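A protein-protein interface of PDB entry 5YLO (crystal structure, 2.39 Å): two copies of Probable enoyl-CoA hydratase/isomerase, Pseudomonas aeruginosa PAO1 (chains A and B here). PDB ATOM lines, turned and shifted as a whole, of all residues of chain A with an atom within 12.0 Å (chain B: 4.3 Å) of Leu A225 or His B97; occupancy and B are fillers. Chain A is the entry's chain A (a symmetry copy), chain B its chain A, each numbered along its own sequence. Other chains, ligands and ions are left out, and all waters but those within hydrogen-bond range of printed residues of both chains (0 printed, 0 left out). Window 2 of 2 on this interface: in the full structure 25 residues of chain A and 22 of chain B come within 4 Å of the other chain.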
ATOM      1  N   LEU A 216      -9.948  -1.621 -10.484  1.00  0.00           N
ATOM      2  CA  LEU A 216     -10.623  -0.336 -10.635  1.00  0.00           C
ATOM      3  C   LEU A 216      -9.910   0.759  -9.857  1.00  0.00           C
ATOM      4  O   LEU A 216      -9.785   1.891 -10.342  1.00  0.00           O
ATOM      5  CB  LEU A 216     -12.079  -0.457 -10.187  1.00  0.00           C
ATOM      6  CG  LEU A 216     -13.007  -1.218 -11.134  1.00  0.00           C
ATOM      7  CD1 LEU A 216     -14.322  -1.532 -10.445  1.00  0.00           C
ATOM      8  CD2 LEU A 216     -13.248  -0.417 -12.406  1.00  0.00           C
ATOM      9  N   LEU A 217      -9.447   0.447  -8.641  1.00  0.00           N
ATOM     10  CA  LEU A 217      -8.666   1.411  -7.872  1.00  0.00           C
ATOM     11  C   LEU A 217      -7.454   1.879  -8.662  1.00  0.00           C
ATOM     12  O   LEU A 217      -7.177   3.080  -8.754  1.00  0.00           O
ATOM     13  CB  LEU A 217      -8.221   0.789  -6.546  1.00  0.00           C
ATOM     14  CG  LEU A 217      -9.266   0.491  -5.471  1.00  0.00           C
ATOM     15  CD1 LEU A 217      -8.710  -0.521  -4.486  1.00  0.00           C
ATOM     16  CD2 LEU A 217      -9.659   1.767  -4.749  1.00  0.00           C
ATOM     17  N   ARG A 218      -6.723   0.933  -9.254  1.00  0.00           N
ATOM     18  CA  ARG A 218      -5.503   1.266  -9.978  1.00  0.00           C
ATOM     19  C   ARG A 218      -5.815   2.031 -11.258  1.00  0.00           C
ATOM     20  O   ARG A 218      -5.208   3.073 -11.532  1.00  0.00           O
ATOM     21  CB  ARG A 218      -4.721  -0.014 -10.276  1.00  0.00           C
ATOM     22  CG  ARG A 218      -3.361   0.191 -10.916  1.00  0.00           C
ATOM     23  CD  ARG A 218      -2.570  -1.113 -10.947  1.00  0.00           C
ATOM     24  NE  ARG A 218      -3.293  -2.188 -11.625  1.00  0.00           N
ATOM     25  CZ  ARG A 218      -3.894  -3.198 -11.001  1.00  0.00           C
ATOM     26  NH1 ARG A 218      -3.859  -3.280  -9.678  1.00  0.00           N
ATOM     27  NH2 ARG A 218      -4.528  -4.127 -11.702  1.00  0.00           N
ATOM     28  N   ASP A 219      -6.769   1.537 -12.052  1.00  0.00           N
ATOM     29  CA  ASP A 219      -7.123   2.228 -13.287  1.00  0.00           C
ATOM     30  C   ASP A 219      -7.743   3.593 -13.015  1.00  0.00           C
ATOM     31  O   ASP A 219      -7.551   4.527 -13.800  1.00  0.00           O
ATOM     32  CB  ASP A 219      -8.083   1.375 -14.120  1.00  0.00           C
ATOM     33  CG  ASP A 219      -7.419   0.146 -14.716  1.00  0.00           C
ATOM     34  OD1 ASP A 219      -6.173   0.061 -14.681  1.00  0.00           O
ATOM     35  OD2 ASP A 219      -8.147  -0.733 -15.227  1.00  0.00           O
ATOM     36  N   GLY A 220      -8.478   3.732 -11.908  1.00  0.00           N
ATOM     37  CA  GLY A 220      -9.166   4.976 -11.607  1.00  0.00           C
ATOM     38  C   GLY A 220      -8.253   6.158 -11.353  1.00  0.00           C
ATOM     39  O   GLY A 220      -8.691   7.304 -11.492  1.00  0.00           O
ATOM     40  N   ALA A 221      -6.996   5.904 -10.981  1.00  0.00           N
ATOM     41  CA  ALA A 221      -6.047   6.984 -10.731  1.00  0.00           C
ATOM     42  C   ALA A 221      -5.726   7.793 -11.981  1.00  0.00           C
ATOM     43  O   ALA A 221      -5.365   8.968 -11.863  1.00  0.00           O
ATOM     44  CB  ALA A 221      -4.758   6.419 -10.136  1.00  0.00           C
ATOM     45  N   GLY A 222      -5.860   7.207 -13.167  1.00  0.00           N
ATOM     46  CA  GLY A 222      -5.519   7.877 -14.401  1.00  0.00           C
ATOM     47  C   GLY A 222      -6.675   8.400 -15.219  1.00  0.00           C
ATOM     48  O   GLY A 222      -6.444   8.946 -16.303  1.00  0.00           O
ATOM     49  N   ARG A 223      -7.911   8.260 -14.745  1.00  0.00           N
ATOM     50  CA  ARG A 223      -9.073   8.736 -15.480  1.00  0.00           C
ATOM     51  C   ARG A 223      -9.988   9.531 -14.555  1.00  0.00           C
ATOM     52  O   ARG A 223      -9.910   9.429 -13.327  1.00  0.00           O
ATOM     53  CB  ARG A 223      -9.843   7.573 -16.128  1.00  0.00           C
ATOM     54  CG  ARG A 223     -10.797   6.857 -15.200  1.00  0.00           C
ATOM     55  CD  ARG A 223     -10.391   5.413 -14.966  1.00  0.00           C
ATOM     56  NE  ARG A 223     -10.392   4.606 -16.185  1.00  0.00           N
ATOM     57  CZ  ARG A 223     -10.625   3.297 -16.209  1.00  0.00           C
ATOM     58  NH1 ARG A 223     -10.898   2.647 -15.085  1.00  0.00           N
ATOM     59  NH2 ARG A 223     -10.602   2.636 -17.358  1.00  0.00           N
ATOM     60  N   SER A 224     -10.854  10.338 -15.165  1.00  0.00           N
ATOM     61  CA  SER A 224     -11.796  11.150 -14.414  1.00  0.00           C
ATOM     62  C   SER A 224     -12.868  10.261 -13.784  1.00  0.00           C
ATOM     63  O   SER A 224     -12.919   9.047 -14.003  1.00  0.00           O
ATOM     64  CB  SER A 224     -12.429  12.204 -15.319  1.00  0.00           C
ATOM     65  OG  SER A 224     -13.281  11.604 -16.282  1.00  0.00           O
ATOM     66  N   LEU A 225     -13.741  10.878 -12.987  1.00  0.00           N
ATOM     67  CA  LEU A 225     -14.844  10.120 -12.412  1.00  0.00           C
ATOM     68  C   LEU A 225     -15.801   9.645 -13.497  1.00  0.00           C
ATOM     69  O   LEU A 225     -16.236   8.488 -13.486  1.00  0.00           O
ATOM     70  CB  LEU A 225     -15.586  10.958 -11.370  1.00  0.00           C
ATOM     71  CG  LEU A 225     -16.842  10.306 -10.784  1.00  0.00           C
ATOM     72  CD1 LEU A 225     -16.502   9.037 -10.013  1.00  0.00           C
ATOM     73  CD2 LEU A 225     -17.595  11.283  -9.903  1.00  0.00           C
ATOM     74  N   ALA A 226     -16.129  10.519 -14.453  1.00  0.00           N
ATOM     75  CA  ALA A 226     -17.044  10.132 -15.523  1.00  0.00           C
ATOM     76  C   ALA A 226     -16.480   8.973 -16.336  1.00  0.00           C
ATOM     77  O   ALA A 226     -17.210   8.036 -16.686  1.00  0.00           O
ATOM     78  CB  ALA A 226     -17.336  11.327 -16.427  1.00  0.00           C
ATOM     79  N   GLU A 227     -15.181   9.015 -16.644  1.00  0.00           N
ATOM     80  CA  GLU A 227     -14.551   7.902 -17.347  1.00  0.00           C
ATOM     81  C   GLU A 227     -14.603   6.626 -16.516  1.00  0.00           C
ATOM     82  O   GLU A 227     -14.920   5.548 -17.031  1.00  0.00           O
ATOM     83  CB  GLU A 227     -13.103   8.247 -17.691  1.00  0.00           C
ATOM     84  CG  GLU A 227     -12.937   9.300 -18.759  1.00  0.00           C
ATOM     85  CD  GLU A 227     -11.520   9.353 -19.290  1.00  0.00           C
ATOM     86  OE1 GLU A 227     -10.614   9.759 -18.532  1.00  0.00           O
ATOM     87  OE2 GLU A 227     -11.314   8.977 -20.462  1.00  0.00           O
ATOM     88  N   GLN A 228     -14.278   6.733 -15.225  1.00  0.00           N
ATOM     89  CA  GLN A 228     -14.315   5.567 -14.348  1.00  0.00           C
ATOM     90  C   GLN A 228     -15.692   4.919 -14.352  1.00  0.00           C
ATOM     91  O   GLN A 228     -15.810   3.689 -14.390  1.00  0.00           O
ATOM     92  CB  GLN A 228     -13.911   5.975 -12.929  1.00  0.00           C
ATOM     93  CG  GLN A 228     -13.997   4.863 -11.889  1.00  0.00           C
ATOM     94  CD  GLN A 228     -12.714   4.057 -11.770  1.00  0.00           C
ATOM     95  OE1 GLN A 228     -11.991   3.873 -12.747  1.00  0.00           O
ATOM     96  NE2 GLN A 228     -12.427   3.578 -10.564  1.00  0.00           N
ATOM     97  N   LEU A 229     -16.751   5.734 -14.336  1.00  0.00           N
ATOM     98  CA  LEU A 229     -18.103   5.187 -14.351  1.00  0.00           C
ATOM     99  C   LEU A 229     -18.428   4.550 -15.697  1.00  0.00           C
ATOM    100  O   LEU A 229     -19.100   3.513 -15.751  1.00  0.00           O
ATOM    101  CB  LEU A 229     -19.115   6.280 -14.004  1.00  0.00           C
ATOM    102  CG  LEU A 229     -18.933   6.948 -12.637  1.00  0.00           C
ATOM    103  CD1 LEU A 229     -20.061   7.928 -12.348  1.00  0.00           C
ATOM    104  CD2 LEU A 229     -18.829   5.906 -11.536  1.00  0.00           C
ATOM    105  N   ARG A 230     -17.964   5.154 -16.796  1.00  0.00           N
ATOM    106  CA  ARG A 230     -18.134   4.528 -18.105  1.00  0.00           C
ATOM    107  C   ARG A 230     -17.432   3.179 -18.162  1.00  0.00           C
ATOM    108  O   ARG A 230     -17.980   2.207 -18.694  1.00  0.00           O
ATOM    109  CB  ARG A 230     -17.598   5.439 -19.213  1.00  0.00           C
ATOM    110  CG  ARG A 230     -18.464   6.640 -19.538  1.00  0.00           C
ATOM    111  CD  ARG A 230     -17.961   7.363 -20.788  1.00  0.00           C
ATOM    112  NE  ARG A 230     -16.567   7.791 -20.671  1.00  0.00           N
ATOM    113  CZ  ARG A 230     -15.588   7.393 -21.479  1.00  0.00           C
ATOM    114  NH1 ARG A 230     -14.351   7.835 -21.297  1.00  0.00           N
ATOM    115  NH2 ARG A 230     -15.845   6.565 -22.483  1.00  0.00           N
ATOM    116  N   ALA A 231     -16.217   3.103 -17.616  1.00  0.00           N
ATOM    117  CA  ALA A 231     -15.446   1.869 -17.706  1.00  0.00           C
ATOM    118  C   ALA A 231     -16.080   0.744 -16.901  1.00  0.00           C
ATOM    119  O   ALA A 231     -15.977  -0.424 -17.290  1.00  0.00           O
ATOM    120  CB  ALA A 231     -14.009   2.112 -17.244  1.00  0.00           C
ATOM    121  N   GLU A 232     -16.742   1.065 -15.791  1.00  0.00           N
ATOM    122  CA  GLU A 232     -17.334   0.026 -14.959  1.00  0.00           C
ATOM    123  C   GLU A 232     -18.665  -0.474 -15.502  1.00  0.00           C
ATOM    124  O   GLU A 232     -19.158  -1.507 -15.037  1.00  0.00           O
ATOM    125  CB  GLU A 232     -17.498   0.535 -13.525  1.00  0.00           C
ATOM    126  CG  GLU A 232     -17.411  -0.556 -12.465  1.00  0.00           C
ATOM    127  CD  GLU A 232     -18.768  -1.123 -12.104  1.00  0.00           C
ATOM    128  OE1 GLU A 232     -19.780  -0.449 -12.384  1.00  0.00           O
ATOM    129  OE2 GLU A 232     -18.825  -2.239 -11.546  1.00  0.00           O
ATOM    130  N   GLN A 233     -19.249   0.215 -16.481  1.00  0.00           N
ATOM    131  CA  GLN A 233     -20.397  -0.302 -17.230  1.00  0.00           C
ATOM    132  C   GLN A 233     -19.976  -1.298 -18.301  1.00  0.00           C
ATOM    133  O   GLN A 233     -20.614  -1.395 -19.355  1.00  0.00           O
ATOM    134  CB  GLN A 233     -21.166   0.862 -17.847  1.00  0.00           C
ATOM    135  CG  GLN A 233     -21.620   1.878 -16.831  1.00  0.00           C
ATOM    136  CD  GLN A 233     -22.421   3.007 -17.441  1.00  0.00           C
ATOM    137  OE1 GLN A 233     -23.466   2.781 -18.051  1.00  0.00           O
ATOM    138  NE2 GLN A 233     -21.934   4.232 -17.284  1.00  0.00           N
ATOM    139  N   ALA A 234     -18.899  -2.036 -18.051  1.00  0.00           N
ATOM    140  CA  ALA A 234     -18.368  -2.995 -19.006  1.00  0.00           C
ATOM    141  C   ALA A 234     -17.430  -3.946 -18.277  1.00  0.00           C
ATOM    142  O   ALA A 234     -16.922  -3.638 -17.196  1.00  0.00           O
ATOM    143  CB  ALA A 234     -17.642  -2.295 -20.159  1.00  0.00           C
ATOM    144  N   MET B  93     -24.164  10.728 -10.312  1.00  0.00           N
ATOM    145  CA  MET B  93     -22.875  10.909  -9.649  1.00  0.00           C
ATOM    146  C   MET B  93     -22.002  11.904 -10.402  1.00  0.00           C
ATOM    147  O   MET B  93     -21.327  12.738  -9.789  1.00  0.00           O
ATOM    148  CB  MET B  93     -22.155   9.568  -9.516  1.00  0.00           C
ATOM    149  CG  MET B  93     -22.918   8.534  -8.719  1.00  0.00           C
ATOM    150  SD  MET B  93     -23.193   9.052  -7.018  1.00  0.00           S
ATOM    151  CE  MET B  93     -23.973   7.582  -6.359  1.00  0.00           C
ATOM    152  N   GLY B  94     -22.013  11.836 -11.735  1.00  0.00           N
ATOM    153  CA  GLY B  94     -21.172  12.725 -12.518  1.00  0.00           C
ATOM    154  C   GLY B  94     -21.550  14.189 -12.387  1.00  0.00           C
ATOM    155  O   GLY B  94     -20.675  15.054 -12.293  1.00  0.00           O
ATOM    156  N   ARG B  95     -22.853  14.469 -12.470  1.00  0.00           N
ATOM    157  CA  ARG B  95     -23.390  15.831 -12.352  1.00  0.00           C
ATOM    158  C   ARG B  95     -23.201  16.474 -10.972  1.00  0.00           C
ATOM    159  O   ARG B  95     -22.823  17.641 -10.871  1.00  0.00           O
ATOM    160  CB  ARG B  95     -24.871  15.853 -12.736  1.00  0.00           C
ATOM    161  CG  ARG B  95     -25.533  17.212 -12.575  1.00  0.00           C
ATOM    162  CD  ARG B  95     -26.993  17.169 -12.997  1.00  0.00           C
ATOM    163  NE  ARG B  95     -27.144  16.817 -14.406  1.00  0.00           N
ATOM    164  CZ  ARG B  95     -27.170  17.702 -15.398  1.00  0.00           C
ATOM    165  NH1 ARG B  95     -27.311  17.292 -16.652  1.00  0.00           N
ATOM    166  NH2 ARG B  95     -27.054  18.997 -15.138  1.00  0.00           N
ATOM    167  N   LEU B  96     -23.465  15.707  -9.918  1.00  0.00           N
ATOM    168  CA  LEU B  96     -23.285  16.182  -8.549  1.00  0.00           C
ATOM    169  C   LEU B  96     -21.818  16.476  -8.270  1.00  0.00           C
ATOM    170  O   LEU B  96     -21.483  17.490  -7.649  1.00  0.00           O
ATOM    171  CB  LEU B  96     -23.822  15.158  -7.550  1.00  0.00           C
ATOM    172  CG  LEU B  96     -23.697  15.564  -6.080  1.00  0.00           C
ATOM    173  CD1 LEU B  96     -24.484  16.839  -5.808  1.00  0.00           C
ATOM    174  CD2 LEU B  96     -24.158  14.436  -5.171  1.00  0.00           C
ATOM    175  N   HIS B  97     -20.930  15.594  -8.730  1.00  0.00           N
ATOM    176  CA  HIS B  97     -19.505  15.763  -8.479  1.00  0.00           C
ATOM    177  C   HIS B  97     -18.962  17.016  -9.155  1.00  0.00           C
ATOM    178  O   HIS B  97     -18.080  17.689  -8.611  1.00  0.00           O
ATOM    179  CB  HIS B  97     -18.758  14.516  -8.953  1.00  0.00           C
ATOM    180  CG  HIS B  97     -17.281  14.705  -9.100  1.00  0.00           C
ATOM    181  ND1 HIS B  97     -16.643  14.659 -10.321  1.00  0.00           N
ATOM    182  CD2 HIS B  97     -16.315  14.933  -8.179  1.00  0.00           C
ATOM    183  CE1 HIS B  97     -15.348  14.856 -10.147  1.00  0.00           C
ATOM    184  NE2 HIS B  97     -15.122  15.025  -8.856  1.00  0.00           N
ATOM    185  N   ALA B  98     -19.484  17.349 -10.335  1.00  0.00           N
ATOM    186  CA  ALA B  98     -19.022  18.491 -11.114  1.00  0.00           C
ATOM    187  C   ALA B  98     -19.953  19.695 -11.017  1.00  0.00           C
ATOM    188  O   ALA B  98     -19.843  20.613 -11.835  1.00  0.00           O
ATOM    189  CB  ALA B  98     -18.846  18.089 -12.579  1.00  0.00           C
ATOM    190  N   LEU B  99     -20.855  19.713 -10.037  1.00  0.00           N
ATOM    191  CA  LEU B  99     -21.838  20.784  -9.924  1.00  0.00           C
ATOM    192  C   LEU B  99     -21.154  22.128  -9.697  1.00  0.00           C
ATOM    193  O   LEU B  99     -20.169  22.227  -8.962  1.00  0.00           O
ATOM    194  CB  LEU B  99     -22.802  20.484  -8.778  1.00  0.00           C
ATOM    195  CG  LEU B  99     -24.124  21.247  -8.778  1.00  0.00           C
ATOM    196  CD1 LEU B  99     -25.145  20.524  -9.646  1.00  0.00           C
ATOM    197  CD2 LEU B  99     -24.639  21.428  -7.360  1.00  0.00           C
ATOM    198  N   CYS B 121     -19.461  12.600  -3.723  1.00  0.00           N
ATOM    199  CA  CYS B 121     -19.563  13.539  -4.832  1.00  0.00           C
ATOM    200  C   CYS B 121     -19.780  14.971  -4.372  1.00  0.00           C
ATOM    201  O   CYS B 121     -19.651  15.895  -5.184  1.00  0.00           O
ATOM    202  CB  CYS B 121     -20.697  13.127  -5.774  1.00  0.00           C
ATOM    203  SG  CYS B 121     -20.441  11.532  -6.600  1.00  0.00           S
ATOM    204  N   TRP B 150     -12.983   5.124  -7.113  1.00  0.00           N
ATOM    205  CA  TRP B 150     -12.453   6.390  -7.596  1.00  0.00           C
ATOM    206  C   TRP B 150     -12.337   7.417  -6.479  1.00  0.00           C
ATOM    207  O   TRP B 150     -11.318   8.106  -6.377  1.00  0.00           O
ATOM    208  CB  TRP B 150     -13.334   6.936  -8.722  1.00  0.00           C
ATOM    209  CG  TRP B 150     -12.708   8.069  -9.489  1.00  0.00           C
ATOM    210  CD1 TRP B 150     -11.961   7.975 -10.631  1.00  0.00           C
ATOM    211  CD2 TRP B 150     -12.778   9.464  -9.170  1.00  0.00           C
ATOM    212  NE1 TRP B 150     -11.561   9.225 -11.039  1.00  0.00           N
ATOM    213  CE2 TRP B 150     -12.050  10.156 -10.161  1.00  0.00           C
ATOM    214  CE3 TRP B 150     -13.385  10.195  -8.145  1.00  0.00           C
ATOM    215  CZ2 TRP B 150     -11.914  11.543 -10.154  1.00  0.00           C
ATOM    216  CZ3 TRP B 150     -13.247  11.572  -8.139  1.00  0.00           C
ATOM    217  CH2 TRP B 150     -12.519  12.232  -9.138  1.00  0.00           C
ATOM    218  N   HIS B 151     -13.359   7.518  -5.627  1.00  0.00           N
ATOM    219  CA  HIS B 151     -13.357   8.509  -4.555  1.00  0.00           C
ATOM    220  C   HIS B 151     -12.451   8.096  -3.402  1.00  0.00           C
ATOM    221  O   HIS B 151     -11.603   8.879  -2.961  1.00  0.00           O
ATOM    222  CB  HIS B 151     -14.780   8.727  -4.041  1.00  0.00           C
ATOM    223  CG  HIS B 151     -15.632   9.559  -4.946  1.00  0.00           C
ATOM    224  ND1 HIS B 151     -15.407  10.904  -5.145  1.00  0.00           N
ATOM    225  CD2 HIS B 151     -16.714   9.243  -5.695  1.00  0.00           C
ATOM    226  CE1 HIS B 151     -16.310  11.380  -5.983  1.00  0.00           C
ATOM    227  NE2 HIS B 151     -17.114  10.393  -6.333  1.00  0.00           N
ATOM    228  N   LYS B 214     -13.697  25.537  -8.591  1.00  0.00           N
ATOM    229  CA  LYS B 214     -14.038  24.120  -8.530  1.00  0.00           C
ATOM    230  C   LYS B 214     -13.689  23.412  -9.834  1.00  0.00           C
ATOM    231  O   LYS B 214     -13.273  22.248  -9.825  1.00  0.00           O
ATOM    232  CB  LYS B 214     -15.520  23.949  -8.193  1.00  0.00           C
ATOM    233  CG  LYS B 214     -15.944  22.505  -7.988  1.00  0.00           C
ATOM    234  CD  LYS B 214     -17.348  22.406  -7.415  1.00  0.00           C
ATOM    235  CE  LYS B 214     -17.806  20.958  -7.340  1.00  0.00           C
ATOM    236  NZ  LYS B 214     -19.117  20.826  -6.643  1.00  0.00           N
ATOM    237  N   ARG B 218     -10.660  20.368 -10.256  1.00  0.00           N
ATOM    238  CA  ARG B 218     -10.935  19.102 -10.924  1.00  0.00           C
ATOM    239  C   ARG B 218     -10.036  18.916 -12.141  1.00  0.00           C
ATOM    240  O   ARG B 218      -9.422  17.857 -12.313  1.00  0.00           O
ATOM    241  CB  ARG B 218     -12.412  19.042 -11.316  1.00  0.00           C
ATOM    242  CG  ARG B 218     -12.873  17.725 -11.908  1.00  0.00           C
ATOM    243  CD  ARG B 218     -14.393  17.686 -12.035  1.00  0.00           C
ATOM    244  NE  ARG B 218     -14.918  18.805 -12.816  1.00  0.00           N
ATOM    245  CZ  ARG B 218     -15.529  19.864 -12.293  1.00  0.00           C
ATOM    246  NH1 ARG B 218     -15.703  19.954 -10.981  1.00  0.00           N
ATOM    247  NH2 ARG B 218     -15.971  20.833 -13.083  1.00  0.00           N
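Of the 19 printed residues of chain A, 6 touch a printed residue of chain B. Hydrophobic or aromatic side chains of chain A within 4 Å of the printed part of chain B: Leu A225 and Leu A229. Of the 12 printed residues of chain B, 4 touch a printed residue of chain A. Hydrophobic or aromatic side chains of chain B within 4 Å of the printed part of chain A: Met B93, His B97, Trp B150 and His B151. Among the printed residues, 8 pairs touch across the chains.
SG of Cys B121 is in hydrogen-bond range of O of Met B93, at 3.5 Å. NE2 of His B151 lies within hydrogen-bond range of SG of Cys B121. The backbone carbonyl oxygen of Leu A216 lies within hydrogen-bond range of the side-chain amide nitrogen of Gln A228 (3.1 Å). The guanidinium group (NH1) of Arg A223 sits at hydrogen-bond distance from the side-chain amide oxygen (OE1) of Gln A228 (2.9 Å). OG of Ser A224 sits at hydrogen-bond distance from N of Glu A227 (3.2 Å). O of Leu A229 lies close to NE2 of Gln A233 (3.3 Å).
Of the printed residues of chain B, Leu A225 touches His B97, Trp B150 and His B151. No residue of chain A comes within 4 Å of Gly B94. No residue of chain A comes within 4 Å of Leu B99. No residue of chain A comes within 4 Å of Cys B121. Trp B150 touches five residues of chain A. No residue of chain A comes within 4 Å of Arg B218. Printed residues of chain B within 4 Å of Arg A223: Trp B150 (2.8 Å). Printed residues of chain B within 4 Å of Leu A229: Met B93. Arg A230 touches none of the printed residues of chain B. The nearest printed residue of chain B that does not touch Leu A225 is Met B93 (4.01 Å). The nearest residue of chain A that does not touch His B97 is Ala A226 (5.9 Å). The nearest printed residue of chain B that does not touch Leu A229 is Gly B94 (4.4 Å).
Among the printed residues, pairs that only touch across the chains: Leu A225 with His B97 (3.5 Å), Leu A225 with His B151 (3.7 Å), Gln A228 with Trp B150 (3.6 Å) and Leu A229 with Met B93 (3.9 Å).
The backbone carbonyl oxygen (O) of Gly A220 lies close to the indole nitrogen (NE1) of Trp B150, 3.5 Å away. The backbone carbonyl oxygen (O) of Arg A223 lies within hydrogen-bond range of the indole nitrogen (NE1) of Trp B150 (2.8 Å). The backbone carbonyl oxygen (O) of Ser A224 sits close to the indole nitrogen (NE1) of Trp B150 (3.3 Å). The indole nitrogen of Trp B150 sits close to the backbone NH of Leu A225.
1 position is printed for both chains. Of the 8 pairs that touch across the chains among the printed residues, none has its exchanged pair printed and touching as well.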
